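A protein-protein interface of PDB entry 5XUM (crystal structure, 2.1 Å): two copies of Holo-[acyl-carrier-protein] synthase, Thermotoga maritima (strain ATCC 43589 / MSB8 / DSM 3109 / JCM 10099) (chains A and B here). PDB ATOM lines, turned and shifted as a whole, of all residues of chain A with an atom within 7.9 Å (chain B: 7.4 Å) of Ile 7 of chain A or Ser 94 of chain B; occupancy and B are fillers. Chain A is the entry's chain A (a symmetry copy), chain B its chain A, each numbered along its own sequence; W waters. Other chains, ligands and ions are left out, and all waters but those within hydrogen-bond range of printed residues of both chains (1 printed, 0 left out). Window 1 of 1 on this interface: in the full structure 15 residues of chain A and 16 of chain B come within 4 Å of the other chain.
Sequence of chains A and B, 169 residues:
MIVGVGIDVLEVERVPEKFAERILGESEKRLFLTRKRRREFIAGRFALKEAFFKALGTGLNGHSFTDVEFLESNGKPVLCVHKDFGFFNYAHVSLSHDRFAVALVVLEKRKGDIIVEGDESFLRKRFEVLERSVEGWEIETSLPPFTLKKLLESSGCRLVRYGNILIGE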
ATOM      1  N   GLY A   4       2.661  -1.374  -2.961  1.00  0.00           N
ATOM      2  CA  GLY A   4       3.037  -0.064  -2.437  1.00  0.00           C
ATOM      3  C   GLY A   4       3.189   0.962  -3.544  1.00  0.00           C
ATOM      4  O   GLY A   4       3.353   0.605  -4.711  1.00  0.00           O
ATOM      5  N   VAL A   5       3.115   2.239  -3.177  1.00  0.00           N
ATOM      6  CA  VAL A   5       3.329   3.339  -4.126  1.00  0.00           C
ATOM      7  C   VAL A   5       4.358   4.327  -3.582  1.00  0.00           C
ATOM      8  O   VAL A   5       4.516   4.467  -2.366  1.00  0.00           O
ATOM      9  CB  VAL A   5       2.021   4.081  -4.507  1.00  0.00           C
ATOM     10  CG1 VAL A   5       1.002   3.123  -5.116  1.00  0.00           C
ATOM     11  CG2 VAL A   5       1.430   4.828  -3.309  1.00  0.00           C
ATOM     12  N   GLY A   6       5.063   4.997  -4.488  1.00  0.00           N
ATOM     13  CA  GLY A   6       6.071   5.969  -4.104  1.00  0.00           C
ATOM     14  C   GLY A   6       6.090   7.131  -5.073  1.00  0.00           C
ATOM     15  O   GLY A   6       5.943   6.946  -6.285  1.00  0.00           O
ATOM     16  N   ILE A   7       6.250   8.330  -4.526  1.00  0.00           N
ATOM     17  CA  ILE A   7       6.379   9.548  -5.317  1.00  0.00           C
ATOM     18  C   ILE A   7       7.609  10.306  -4.796  1.00  0.00           C
ATOM     19  O   ILE A   7       7.903  10.269  -3.599  1.00  0.00           O
ATOM     20  CB  ILE A   7       5.086  10.415  -5.245  1.00  0.00           C
ATOM     21  CG1 ILE A   7       5.049  11.472  -6.356  1.00  0.00           C
ATOM     22  CG2 ILE A   7       4.938  11.101  -3.889  1.00  0.00           C
ATOM     23  CD1 ILE A   7       4.450  11.004  -7.662  1.00  0.00           C
ATOM     24  N   ASP A   8       8.348  10.951  -5.692  1.00  0.00           N
ATOM     25  CA  ASP A   8       9.467  11.800  -5.279  1.00  0.00           C
ATOM     26  C   ASP A   8       9.599  13.028  -6.165  1.00  0.00           C
ATOM     27  O   ASP A   8       9.487  12.929  -7.385  1.00  0.00           O
ATOM     28  CB  ASP A   8      10.793  11.032  -5.256  1.00  0.00           C
ATOM     29  CG  ASP A   8      11.853  11.728  -4.406  1.00  0.00           C
ATOM     30  OD1 ASP A   8      12.951  12.026  -4.928  1.00  0.00           O
ATOM     31  OD2 ASP A   8      11.586  11.984  -3.211  1.00  0.00           O
ATOM     32  N   VAL A   9       9.835  14.178  -5.539  1.00  0.00           N
ATOM     33  CA  VAL A   9      10.056  15.434  -6.255  1.00  0.00           C
ATOM     34  C   VAL A   9      11.408  16.036  -5.853  1.00  0.00           C
ATOM     35  O   VAL A   9      11.748  16.073  -4.670  1.00  0.00           O
ATOM     36  CB  VAL A   9       8.883  16.435  -6.040  1.00  0.00           C
ATOM     37  CG1 VAL A   9       8.753  16.854  -4.581  1.00  0.00           C
ATOM     38  CG2 VAL A   9       9.015  17.657  -6.948  1.00  0.00           C
ATOM     39  N   ALA A  47      15.530  10.396  -8.024  1.00  0.00           N
ATOM     40  CA  ALA A  47      14.094  10.475  -7.768  1.00  0.00           C
ATOM     41  C   ALA A  47      13.409   9.110  -7.893  1.00  0.00           C
ATOM     42  O   ALA A  47      12.570   8.765  -7.066  1.00  0.00           O
ATOM     43  CB  ALA A  47      13.438  11.497  -8.691  1.00  0.00           C
ATOM     44  N   LEU A  48      13.773   8.344  -8.919  1.00  0.00           N
ATOM     45  CA  LEU A  48      13.225   6.997  -9.122  1.00  0.00           C
ATOM     46  C   LEU A  48      13.580   6.039  -7.983  1.00  0.00           C
ATOM     47  O   LEU A  48      12.728   5.271  -7.525  1.00  0.00           O
ATOM     48  CB  LEU A  48      13.669   6.419 -10.473  1.00  0.00           C
ATOM     49  CG  LEU A  48      12.914   6.920 -11.709  1.00  0.00           C
ATOM     50  CD1 LEU A  48      13.716   6.678 -12.982  1.00  0.00           C
ATOM     51  CD2 LEU A  48      11.533   6.282 -11.805  1.00  0.00           C
ATOM     52  N   GLU A  50      14.481   6.914  -4.844  1.00  0.00           N
ATOM     53  CA  GLU A  50      13.746   7.406  -3.676  1.00  0.00           C
ATOM     54  C   GLU A  50      12.283   6.961  -3.699  1.00  0.00           C
ATOM     55  O   GLU A  50      11.770   6.467  -2.696  1.00  0.00           O
ATOM     56  CB  GLU A  50      13.827   8.935  -3.580  1.00  0.00           C
ATOM     57  CG  GLU A  50      15.131   9.472  -3.012  1.00  0.00           C
ATOM     58  CD  GLU A  50      15.181   9.418  -1.494  1.00  0.00           C
ATOM     59  OE1 GLU A  50      15.026  10.480  -0.857  1.00  0.00           O
ATOM     60  OE2 GLU A  50      15.367   8.317  -0.935  1.00  0.00           O
ATOM     61  N   ALA A  51      11.623   7.138  -4.845  1.00  0.00           N
ATOM     62  CA  ALA A  51      10.247   6.667  -5.031  1.00  0.00           C
ATOM     63  C   ALA A  51      10.118   5.153  -4.825  1.00  0.00           C
ATOM     64  O   ALA A  51       9.145   4.689  -4.225  1.00  0.00           O
ATOM     65  CB  ALA A  51       9.719   7.067  -6.401  1.00  0.00           C
ATOM     66  N   PHE A  52      11.099   4.393  -5.312  1.00  0.00           N
ATOM     67  CA  PHE A  52      11.104   2.934  -5.136  1.00  0.00           C
ATOM     68  C   PHE A  52      11.133   2.537  -3.659  1.00  0.00           C
ATOM     69  O   PHE A  52      10.319   1.727  -3.214  1.00  0.00           O
ATOM     70  CB  PHE A  52      12.261   2.275  -5.902  1.00  0.00           C
ATOM     71  CG  PHE A  52      12.390   0.793  -5.649  1.00  0.00           C
ATOM     72  CD1 PHE A  52      11.492  -0.108  -6.218  1.00  0.00           C
ATOM     73  CD2 PHE A  52      13.404   0.298  -4.830  1.00  0.00           C
ATOM     74  CE1 PHE A  52      11.607  -1.474  -5.979  1.00  0.00           C
ATOM     75  CE2 PHE A  52      13.523  -1.066  -4.589  1.00  0.00           C
ATOM     76  CZ  PHE A  52      12.625  -1.954  -5.165  1.00  0.00           C
ATOM     77  N   PHE A  53      12.061   3.112  -2.898  1.00  0.00           N
ATOM     78  CA  PHE A  53      12.170   2.791  -1.477  1.00  0.00           C
ATOM     79  C   PHE A  53      10.975   3.263  -0.650  1.00  0.00           C
ATOM     80  O   PHE A  53      10.638   2.639   0.355  1.00  0.00           O
ATOM     81  CB  PHE A  53      13.500   3.278  -0.893  1.00  0.00           C
ATOM     82  CG  PHE A  53      14.686   2.483  -1.364  1.00  0.00           C
ATOM     83  CD1 PHE A  53      14.855   1.159  -0.966  1.00  0.00           C
ATOM     84  CD2 PHE A  53      15.627   3.048  -2.210  1.00  0.00           C
ATOM     85  CE1 PHE A  53      15.943   0.420  -1.405  1.00  0.00           C
ATOM     86  CE2 PHE A  53      16.717   2.313  -2.653  1.00  0.00           C
ATOM     87  CZ  PHE A  53      16.876   1.001  -2.247  1.00  0.00           C
ATOM     88  N   LYS A  54      10.333   4.350  -1.083  1.00  0.00           N
ATOM     89  CA  LYS A  54       9.071   4.799  -0.487  1.00  0.00           C
ATOM     90  C   LYS A  54       7.955   3.776  -0.713  1.00  0.00           C
ATOM     91  O   LYS A  54       7.142   3.530   0.180  1.00  0.00           O
ATOM     92  CB  LYS A  54       8.641   6.161  -1.048  1.00  0.00           C
ATOM     93  CG  LYS A  54       9.406   7.358  -0.499  1.00  0.00           C
ATOM     94  CD  LYS A  54       8.659   8.645  -0.815  1.00  0.00           C
ATOM     95  CE  LYS A  54       9.377   9.875  -0.285  1.00  0.00           C
ATOM     96  NZ  LYS A  54      10.409  10.355  -1.241  1.00  0.00           N
ATOM     97  N   ALA A  55       7.927   3.193  -1.911  1.00  0.00           N
ATOM     98  CA  ALA A  55       6.946   2.161  -2.270  1.00  0.00           C
ATOM     99  C   ALA A  55       7.096   0.869  -1.450  1.00  0.00           C
ATOM    100  O   ALA A  55       6.109   0.176  -1.197  1.00  0.00           O
ATOM    101  CB  ALA A  55       7.013   1.864  -3.763  1.00  0.00           C
ATOM    102  N   SER A  94       7.339   5.646 -13.755  1.00  0.00           N
ATOM    103  CA  SER A  94       7.311   6.780 -14.670  1.00  0.00           C
ATOM    104  C   SER A  94       8.161   7.915 -14.119  1.00  0.00           C
ATOM    105  O   SER A  94       8.282   8.078 -12.902  1.00  0.00           O
ATOM    106  CB  SER A  94       5.878   7.257 -14.915  1.00  0.00           C
ATOM    107  OG  SER A  94       5.834   8.189 -15.991  1.00  0.00           O
ATOM    108  N   ALA A 101      12.176  17.364 -11.121  1.00  0.00           N
ATOM    109  CA  ALA A 101      11.952  15.985 -11.535  1.00  0.00           C
ATOM    110  C   ALA A 101      10.892  15.351 -10.641  1.00  0.00           C
ATOM    111  O   ALA A 101      10.912  15.538  -9.426  1.00  0.00           O
ATOM    112  CB  ALA A 101      13.248  15.193 -11.474  1.00  0.00           C
ATOM    113  N   VAL A 102       9.950  14.630 -11.245  1.00  0.00           N
ATOM    114  CA  VAL A 102       8.945  13.876 -10.488  1.00  0.00           C
ATOM    115  C   VAL A 102       8.956  12.414 -10.933  1.00  0.00           C
ATOM    116  O   VAL A 102       8.803  12.113 -12.123  1.00  0.00           O
ATOM    117  CB  VAL A 102       7.522  14.478 -10.607  1.00  0.00           C
ATOM    118  CG1 VAL A 102       6.512  13.656  -9.809  1.00  0.00           C
ATOM    119  CG2 VAL A 102       7.501  15.925 -10.126  1.00  0.00           C
ATOM    120  N   ALA A 103       9.152  11.516  -9.971  1.00  0.00           N
ATOM    121  CA  ALA A 103       9.185  10.082 -10.245  1.00  0.00           C
ATOM    122  C   ALA A 103       8.052   9.356  -9.533  1.00  0.00           C
ATOM    123  O   ALA A 103       7.700   9.691  -8.402  1.00  0.00           O
ATOM    124  CB  ALA A 103      10.521   9.493  -9.842  1.00  0.00           C
ATOM    125  N   LEU A 104       7.497   8.362 -10.217  1.00  0.00           N
ATOM    126  CA  LEU A 104       6.392   7.558  -9.713  1.00  0.00           C
ATOM    127  C   LEU A 104       6.755   6.074  -9.794  1.00  0.00           C
ATOM    128  O   LEU A 104       7.219   5.601 -10.829  1.00  0.00           O
ATOM    129  CB  LEU A 104       5.133   7.833 -10.544  1.00  0.00           C
ATOM    130  CG  LEU A 104       3.917   6.912 -10.372  1.00  0.00           C
ATOM    131  CD1 LEU A 104       3.233   7.172  -9.041  1.00  0.00           C
ATOM    132  CD2 LEU A 104       2.939   7.109 -11.518  1.00  0.00           C
ATOM    133  N   VAL A 105       6.554   5.353  -8.692  1.00  0.00           N
ATOM    134  CA  VAL A 105       6.747   3.901  -8.664  1.00  0.00           C
ATOM    135  C   VAL A 105       5.506   3.252  -8.048  1.00  0.00           C
ATOM    136  O   VAL A 105       5.086   3.617  -6.946  1.00  0.00           O
ATOM    137  CB  VAL A 105       8.024   3.485  -7.890  1.00  0.00           C
ATOM    138  CG1 VAL A 105       8.114   1.964  -7.742  1.00  0.00           C
ATOM    139  CG2 VAL A 105       9.276   4.007  -8.584  1.00  0.00           C
ATOM    140  N   VAL A 106       4.909   2.316  -8.782  1.00  0.00           N
ATOM    141  CA  VAL A 106       3.792   1.523  -8.271  1.00  0.00           C
ATOM    142  C   VAL A 106       4.178   0.047  -8.323  1.00  0.00           C
ATOM    143  O   VAL A 106       4.450  -0.499  -9.397  1.00  0.00           O
ATOM    144  CB  VAL A 106       2.479   1.773  -9.054  1.00  0.00           C
ATOM    145  CG1 VAL A 106       1.369   0.850  -8.552  1.00  0.00           C
ATOM    146  CG2 VAL A 106       2.039   3.235  -8.938  1.00  0.00           C
ATOM    147  N   GLY B   6      -5.390  10.094  -6.800  1.00  0.00           N
ATOM    148  CA  GLY B   6      -5.328  11.527  -6.574  1.00  0.00           C
ATOM    149  C   GLY B   6      -3.890  11.995  -6.514  1.00  0.00           C
ATOM    150  O   GLY B   6      -3.026  11.316  -5.952  1.00  0.00           O
ATOM    151  N   ILE B   7      -3.640  13.152  -7.116  1.00  0.00           N
ATOM    152  CA  ILE B   7      -2.332  13.795  -7.080  1.00  0.00           C
ATOM    153  C   ILE B   7      -2.550  15.258  -6.668  1.00  0.00           C
ATOM    154  O   ILE B   7      -3.565  15.861  -7.024  1.00  0.00           O
ATOM    155  CB  ILE B   7      -1.600  13.677  -8.450  1.00  0.00           C
ATOM    156  CG1 ILE B   7      -0.103  13.984  -8.323  1.00  0.00           C
ATOM    157  CG2 ILE B   7      -2.218  14.595  -9.503  1.00  0.00           C
ATOM    158  CD1 ILE B   7       0.764  12.801  -7.961  1.00  0.00           C
ATOM    159  N   GLY B  44       2.435  19.436   3.485  1.00  0.00           N
ATOM    160  CA  GLY B  44       2.323  18.015   3.169  1.00  0.00           C
ATOM    161  C   GLY B  44       0.963  17.420   3.500  1.00  0.00           C
ATOM    162  O   GLY B  44       0.409  16.654   2.709  1.00  0.00           O
ATOM    163  N   ALA B  47      -1.666  18.764   1.084  1.00  0.00           N
ATOM    164  CA  ALA B  47      -1.514  18.070  -0.192  1.00  0.00           C
ATOM    165  C   ALA B  47      -2.079  16.647  -0.148  1.00  0.00           C
ATOM    166  O   ALA B  47      -2.749  16.221  -1.085  1.00  0.00           O
ATOM    167  CB  ALA B  47      -0.053  18.061  -0.628  1.00  0.00           C
ATOM    168  N   LEU B  48      -1.811  15.925   0.939  1.00  0.00           N
ATOM    169  CA  LEU B  48      -2.334  14.566   1.122  1.00  0.00           C
ATOM    170  C   LEU B  48      -3.862  14.526   1.191  1.00  0.00           C
ATOM    171  O   LEU B  48      -4.493  13.652   0.588  1.00  0.00           O
ATOM    172  CB  LEU B  48      -1.720  13.901   2.361  1.00  0.00           C
ATOM    173  CG  LEU B  48      -0.301  13.343   2.202  1.00  0.00           C
ATOM    174  CD1 LEU B  48       0.375  13.158   3.554  1.00  0.00           C
ATOM    175  CD2 LEU B  48      -0.312  12.037   1.415  1.00  0.00           C
ATOM    176  N   ALA B  51      -5.238  15.351  -2.318  1.00  0.00           N
ATOM    177  CA  ALA B  51      -5.080  14.133  -3.120  1.00  0.00           C
ATOM    178  C   ALA B  51      -6.108  13.057  -2.751  1.00  0.00           C
ATOM    179  O   ALA B  51      -6.643  12.381  -3.634  1.00  0.00           O
ATOM    180  CB  ALA B  51      -3.666  13.585  -2.997  1.00  0.00           C
ATOM    181  N   PHE B  70      -3.681  12.025   8.374  1.00  0.00           N
ATOM    182  CA  PHE B  70      -2.509  11.297   7.924  1.00  0.00           C
ATOM    183  C   PHE B  70      -1.480  11.256   9.040  1.00  0.00           C
ATOM    184  O   PHE B  70      -0.794  12.247   9.320  1.00  0.00           O
ATOM    185  CB  PHE B  70      -1.944  11.894   6.633  1.00  0.00           C
ATOM    186  CG  PHE B  70      -2.839  11.696   5.441  1.00  0.00           C
ATOM    187  CD1 PHE B  70      -2.688  10.585   4.622  1.00  0.00           C
ATOM    188  CD2 PHE B  70      -3.843  12.612   5.148  1.00  0.00           C
ATOM    189  CE1 PHE B  70      -3.513  10.396   3.522  1.00  0.00           C
ATOM    190  CE2 PHE B  70      -4.674  12.427   4.054  1.00  0.00           C
ATOM    191  CZ  PHE B  70      -4.508  11.318   3.239  1.00  0.00           C
ATOM    192  N   LYS B  76       6.442   6.525   6.948  1.00  0.00           N
ATOM    193  CA  LYS B  76       5.414   6.636   5.916  1.00  0.00           C
ATOM    194  C   LYS B  76       4.097   7.184   6.483  1.00  0.00           C
ATOM    195  O   LYS B  76       3.677   6.783   7.572  1.00  0.00           O
ATOM    196  CB  LYS B  76       5.190   5.268   5.252  1.00  0.00           C
ATOM    197  CG  LYS B  76       4.159   5.256   4.127  1.00  0.00           C
ATOM    198  CD  LYS B  76       3.920   3.860   3.565  1.00  0.00           C
ATOM    199  CE  LYS B  76       4.870   3.548   2.419  1.00  0.00           C
ATOM    200  NZ  LYS B  76       4.562   2.252   1.747  1.00  0.00           N
ATOM    201  N   PRO B  77       3.446   8.109   5.747  1.00  0.00           N
ATOM    202  CA  PRO B  77       2.103   8.558   6.118  1.00  0.00           C
ATOM    203  C   PRO B  77       1.100   7.409   6.058  1.00  0.00           C
ATOM    204  O   PRO B  77       1.214   6.536   5.194  1.00  0.00           O
ATOM    205  CB  PRO B  77       1.765   9.600   5.046  1.00  0.00           C
ATOM    206  CG  PRO B  77       3.078  10.047   4.509  1.00  0.00           C
ATOM    207  CD  PRO B  77       3.960   8.836   4.570  1.00  0.00           C
ATOM    208  N   ALA B  91      -5.540   2.234   1.278  1.00  0.00           N
ATOM    209  CA  ALA B  91      -5.111   3.539   0.808  1.00  0.00           C
ATOM    210  C   ALA B  91      -3.594   3.525   0.736  1.00  0.00           C
ATOM    211  O   ALA B  91      -2.911   3.459   1.758  1.00  0.00           O
ATOM    212  CB  ALA B  91      -5.597   4.638   1.740  1.00  0.00           C
ATOM    213  N   HIS B  92      -3.079   3.546  -0.485  1.00  0.00           N
ATOM    214  CA  HIS B  92      -1.649   3.591  -0.713  1.00  0.00           C
ATOM    215  C   HIS B  92      -1.274   5.021  -0.941  1.00  0.00           C
ATOM    216  O   HIS B  92      -1.716   5.651  -1.910  1.00  0.00           O
ATOM    217  CB  HIS B  92      -1.279   2.707  -1.897  1.00  0.00           C
ATOM    218  CG  HIS B  92      -1.712   1.268  -1.734  1.00  0.00           C
ATOM    219  ND1 HIS B  92      -1.043   0.393  -0.956  1.00  0.00           N
ATOM    220  CD2 HIS B  92      -2.794   0.570  -2.273  1.00  0.00           C
ATOM    221  CE1 HIS B  92      -1.659  -0.805  -1.000  1.00  0.00           C
ATOM    222  NE2 HIS B  92      -2.730  -0.695  -1.805  1.00  0.00           N
ATOM    223  N   VAL B  93      -0.478   5.561  -0.023  1.00  0.00           N
ATOM    224  CA  VAL B  93      -0.174   6.987  -0.025  1.00  0.00           C
ATOM    225  C   VAL B  93       1.334   7.252  -0.033  1.00  0.00           C
ATOM    226  O   VAL B  93       2.125   6.452   0.473  1.00  0.00           O
ATOM    227  CB  VAL B  93      -0.875   7.751   1.139  1.00  0.00           C
ATOM    228  CG1 VAL B  93      -2.371   7.456   1.166  1.00  0.00           C
ATOM    229  CG2 VAL B  93      -0.250   7.419   2.484  1.00  0.00           C
ATOM    230  N   SER B  94       1.719   8.368  -0.639  1.00  0.00           N
ATOM    231  CA  SER B  94       3.107   8.811  -0.631  1.00  0.00           C
ATOM    232  C   SER B  94       3.170  10.330  -0.673  1.00  0.00           C
ATOM    233  O   SER B  94       2.294  10.981  -1.249  1.00  0.00           O
ATOM    234  CB  SER B  94       3.885   8.212  -1.805  1.00  0.00           C
ATOM    235  OG  SER B  94       5.281   8.440  -1.654  1.00  0.00           O
ATOM    236  N   LEU B  95       4.212  10.877  -0.055  1.00  0.00           N
ATOM    237  CA  LEU B  95       4.429  12.314   0.006  1.00  0.00           C
ATOM    238  C   LEU B  95       5.909  12.628  -0.174  1.00  0.00           C
ATOM    239  O   LEU B  95       6.772  11.965   0.407  1.00  0.00           O
ATOM    240  CB  LEU B  95       3.932  12.879   1.344  1.00  0.00           C
ATOM    241  CG  LEU B  95       4.302  14.327   1.694  1.00  0.00           C
ATOM    242  CD1 LEU B  95       3.485  15.325   0.874  1.00  0.00           C
ATOM    243  CD2 LEU B  95       4.134  14.579   3.185  1.00  0.00           C
ATOM    244  N   SER B  96       6.186  13.639  -0.987  1.00  0.00           N
ATOM    245  CA  SER B  96       7.536  14.155  -1.163  1.00  0.00           C
ATOM    246  C   SER B  96       7.478  15.677  -1.198  1.00  0.00           C
ATOM    247  O   SER B  96       6.477  16.252  -1.630  1.00  0.00           O
ATOM    248  CB  SER B  96       8.133  13.624  -2.465  1.00  0.00           C
ATOM    249  OG  SER B  96       9.495  13.990  -2.593  1.00  0.00           O
ATOM    250  N   HIS B  97       8.535  16.330  -0.727  1.00  0.00           N
ATOM    251  CA  HIS B  97       8.644  17.784  -0.868  1.00  0.00           C
ATOM    252  C   HIS B  97      10.049  18.267  -1.062  1.00  0.00           C
ATOM    253  O   HIS B  97      10.972  17.831  -0.371  1.00  0.00           O
ATOM    254  CB  HIS B  97       7.951  18.555   0.267  1.00  0.00           C
ATOM    255  CG  HIS B  97       8.062  17.902   1.623  1.00  0.00           C
ATOM    256  ND1 HIS B  97       9.240  17.722   2.247  1.00  0.00           N
ATOM    257  CD2 HIS B  97       7.080  17.410   2.483  1.00  0.00           C
ATOM    258  CE1 HIS B  97       9.030  17.126   3.437  1.00  0.00           C
ATOM    259  NE2 HIS B  97       7.705  16.937   3.579  1.00  0.00           N
ATOM    260  N   VAL B 102       4.529  17.262  -3.252  1.00  0.00           N
ATOM    261  CA  VAL B 102       3.706  16.421  -4.130  1.00  0.00           C
ATOM    262  C   VAL B 102       3.185  15.216  -3.346  1.00  0.00           C
ATOM    263  O   VAL B 102       3.965  14.458  -2.757  1.00  0.00           O
ATOM    264  CB  VAL B 102       4.457  15.965  -5.407  1.00  0.00           C
ATOM    265  CG1 VAL B 102       3.563  15.088  -6.283  1.00  0.00           C
ATOM    266  CG2 VAL B 102       4.944  17.166  -6.210  1.00  0.00           C
ATOM    267  N   ALA B 103       1.864  15.059  -3.335  1.00  0.00           N
ATOM    268  CA  ALA B 103       1.222  13.953  -2.630  1.00  0.00           C
ATOM    269  C   ALA B 103       0.479  13.038  -3.595  1.00  0.00           C
ATOM    270  O   ALA B 103      -0.129  13.501  -4.561  1.00  0.00           O
ATOM    271  CB  ALA B 103       0.276  14.474  -1.568  1.00  0.00           C
ATOM    272  N   LEU B 104       0.541  11.742  -3.310  1.00  0.00           N
ATOM    273  CA  LEU B 104      -0.093  10.710  -4.119  1.00  0.00           C
ATOM    274  C   LEU B 104      -0.985   9.837  -3.236  1.00  0.00           C
ATOM    275  O   LEU B 104      -0.557   9.379  -2.177  1.00  0.00           O
ATOM    276  CB  LEU B 104       0.984   9.847  -4.789  1.00  0.00           C
ATOM    277  CG  LEU B 104       0.562   8.541  -5.474  1.00  0.00           C
ATOM    278  CD1 LEU B 104      -0.173   8.828  -6.771  1.00  0.00           C
ATOM    279  CD2 LEU B 104       1.778   7.667  -5.738  1.00  0.00           C
ATOM    280  N   VAL B 105      -2.226   9.624  -3.670  1.00  0.00           N
ATOM    281  CA  VAL B 105      -3.147   8.715  -2.986  1.00  0.00           C
ATOM    282  C   VAL B 105      -3.748   7.756  -4.016  1.00  0.00           C
ATOM    283  O   VAL B 105      -4.299   8.188  -5.032  1.00  0.00           O
ATOM    284  CB  VAL B 105      -4.266   9.467  -2.220  1.00  0.00           C
ATOM    285  CG1 VAL B 105      -5.301   8.493  -1.650  1.00  0.00           C
ATOM    286  CG2 VAL B 105      -3.684  10.313  -1.096  1.00  0.00           C
ATOM    287  N   VAL B 106      -3.604   6.457  -3.760  1.00  0.00           N
ATOM    288  CA  VAL B 106      -4.232   5.428  -4.587  1.00  0.00           C
ATOM    289  C   VAL B 106      -5.148   4.585  -3.703  1.00  0.00           C
ATOM    290  O   VAL B 106      -4.694   3.948  -2.747  1.00  0.00           O
ATOM    291  CB  VAL B 106      -3.198   4.534  -5.313  1.00  0.00           C
ATOM    292  CG1 VAL B 106      -3.899   3.414  -6.080  1.00  0.00           C
ATOM    293  CG2 VAL B 106      -2.329   5.360  -6.266  1.00  0.00           C
HETATM  294  O   HOH W   1       2.820   2.912  -0.317  1.00  0.00           O
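Water W1 bridges NZ of Lys 76 of chain B and N of Val 5 of chain A.
Of the printed residues of chain B, Gly 6 of chain A touches Ser 94. Ile 7 of chain A touches just these residues of chain B: Ser 94 (3.0 Å), Leu 95 (3.9 Å), Ser 96 (3.5 Å) and Val 102 (3.7 Å). Ala 91 of chain B touches none of the printed residues of chain A. Of chain A, only Val 5, Gly 6, Ile 7 and Lys 54 come within 4 Å of Ser 94 of chain B. Of the printed residues of chain A, Leu 95 of chain B touches Ile 7 and Lys 54. The nearest residue of chain B that does not touch Ile 7 of chain A is Ile 7 of chain B (4.1 Å). The nearest printed residue of chain B that does not touch Val 5 of chain A is Val 106 of chain B (4.2 Å).
Among the printed residues, pairs that only touch across the chains: Val 5 of chain A with His 92 of chain B (3.5 Å), Val 5 of chain A with Val 93 of chain B (3.9 Å), Val 5 of chain A with Ser 94 of chain B (3.8 Å), Val 5 of chain A with Leu 104 of chain B (3.8 Å), Gly 6 of chain A with Ser 94 of chain B (3.6 Å), Ile 7 of chain A with Leu 95 of chain B (3.9 Å), Ile 7 of chain A with Ser 96 of chain B (3.5 Å), Ile 7 of chain A with Val 102 of chain B (3.7 Å), Val 9 of chain A with His 97 of chain B (3.8 Å), Lys 54 of chain A with Ser 94 of chain B (3.5 Å), Lys 54 of chain A with Leu 95 of chain B (3.4 Å), Lys 54 of chain A with Ser 96 of chain B (3.98 Å), Ala 55 of chain A with Lys 76 of chain B (3.9 Å) and Leu 104 of chain A with Leu 104 of chain B (3.6 Å).
O of Ser 96 of chain B sits at hydrogen-bond distance from N of Val 102 of chain B. O of Ser 94 of chain A sits at hydrogen-bond distance from N of Leu 104 of chain A (2.8 Å). O of Ile 7 of chain A lies close to NZ of Lys 54 of chain A, 3.4 Å away. OD2 of Asp 8 of chain A is in salt-bridge range of NZ of Lys 54 of chain A (2.8 Å). O of Asp 8 of chain A lies within hydrogen-bond range of N of Ala 103 of chain A. O of His 92 of chain B is in hydrogen-bond range of N of Val 106 of chain B, at 2.8 Å.
Of the 21 printed residues of chain A, 8 touch a printed residue of chain B. Of the 21 printed residues of chain B, 9 touch a printed residue of chain A. Hydrophobic or aromatic side chains of chain B that line the printed part of chain A: His 92, Val 102 and Leu 104. Among the printed residues, no Asp or Glu carboxylate lies within 4 Å of a Lys or Arg side-chain nitrogen of the other chain.
Gly 6 of chain A touches Ser 94 of chain B, but with the chains exchanged Ser 94 of chain A does not touch Gly 6 of chain B (13.3 Å). Ile 7 of chain A touches Ser 94 of chain B, but with the chains exchanged Ser 94 of chain A does not touch Ile 7 of chain B (10.2 Å). Ile 7 of chain A touches Val 102 of chain B, but with the chains exchanged Val 102 of chain A does not touch Ile 7 of chain B (6.1 Å). Leu 104 of chain B touches its own counterpart, Leu 104 of chain A. 11 positions are printed for both chains.
The side-chain carboxylate (OD2) of Asp 8 of chain A lies within hydrogen-bond range of the side-chain hydroxyl (OG) of Ser 96 of chain B. OG of Ser 94 of chain B is in hydrogen-bond range of N of Ile 7 of chain A (3.0 Å). NZ of Lys 76 of chain B lies close to O of Lys 54 of chain A (3.3 Å). OG of Ser 96 of chain B is in hydrogen-bond range of N of Val 9 of chain A (3.0 Å).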
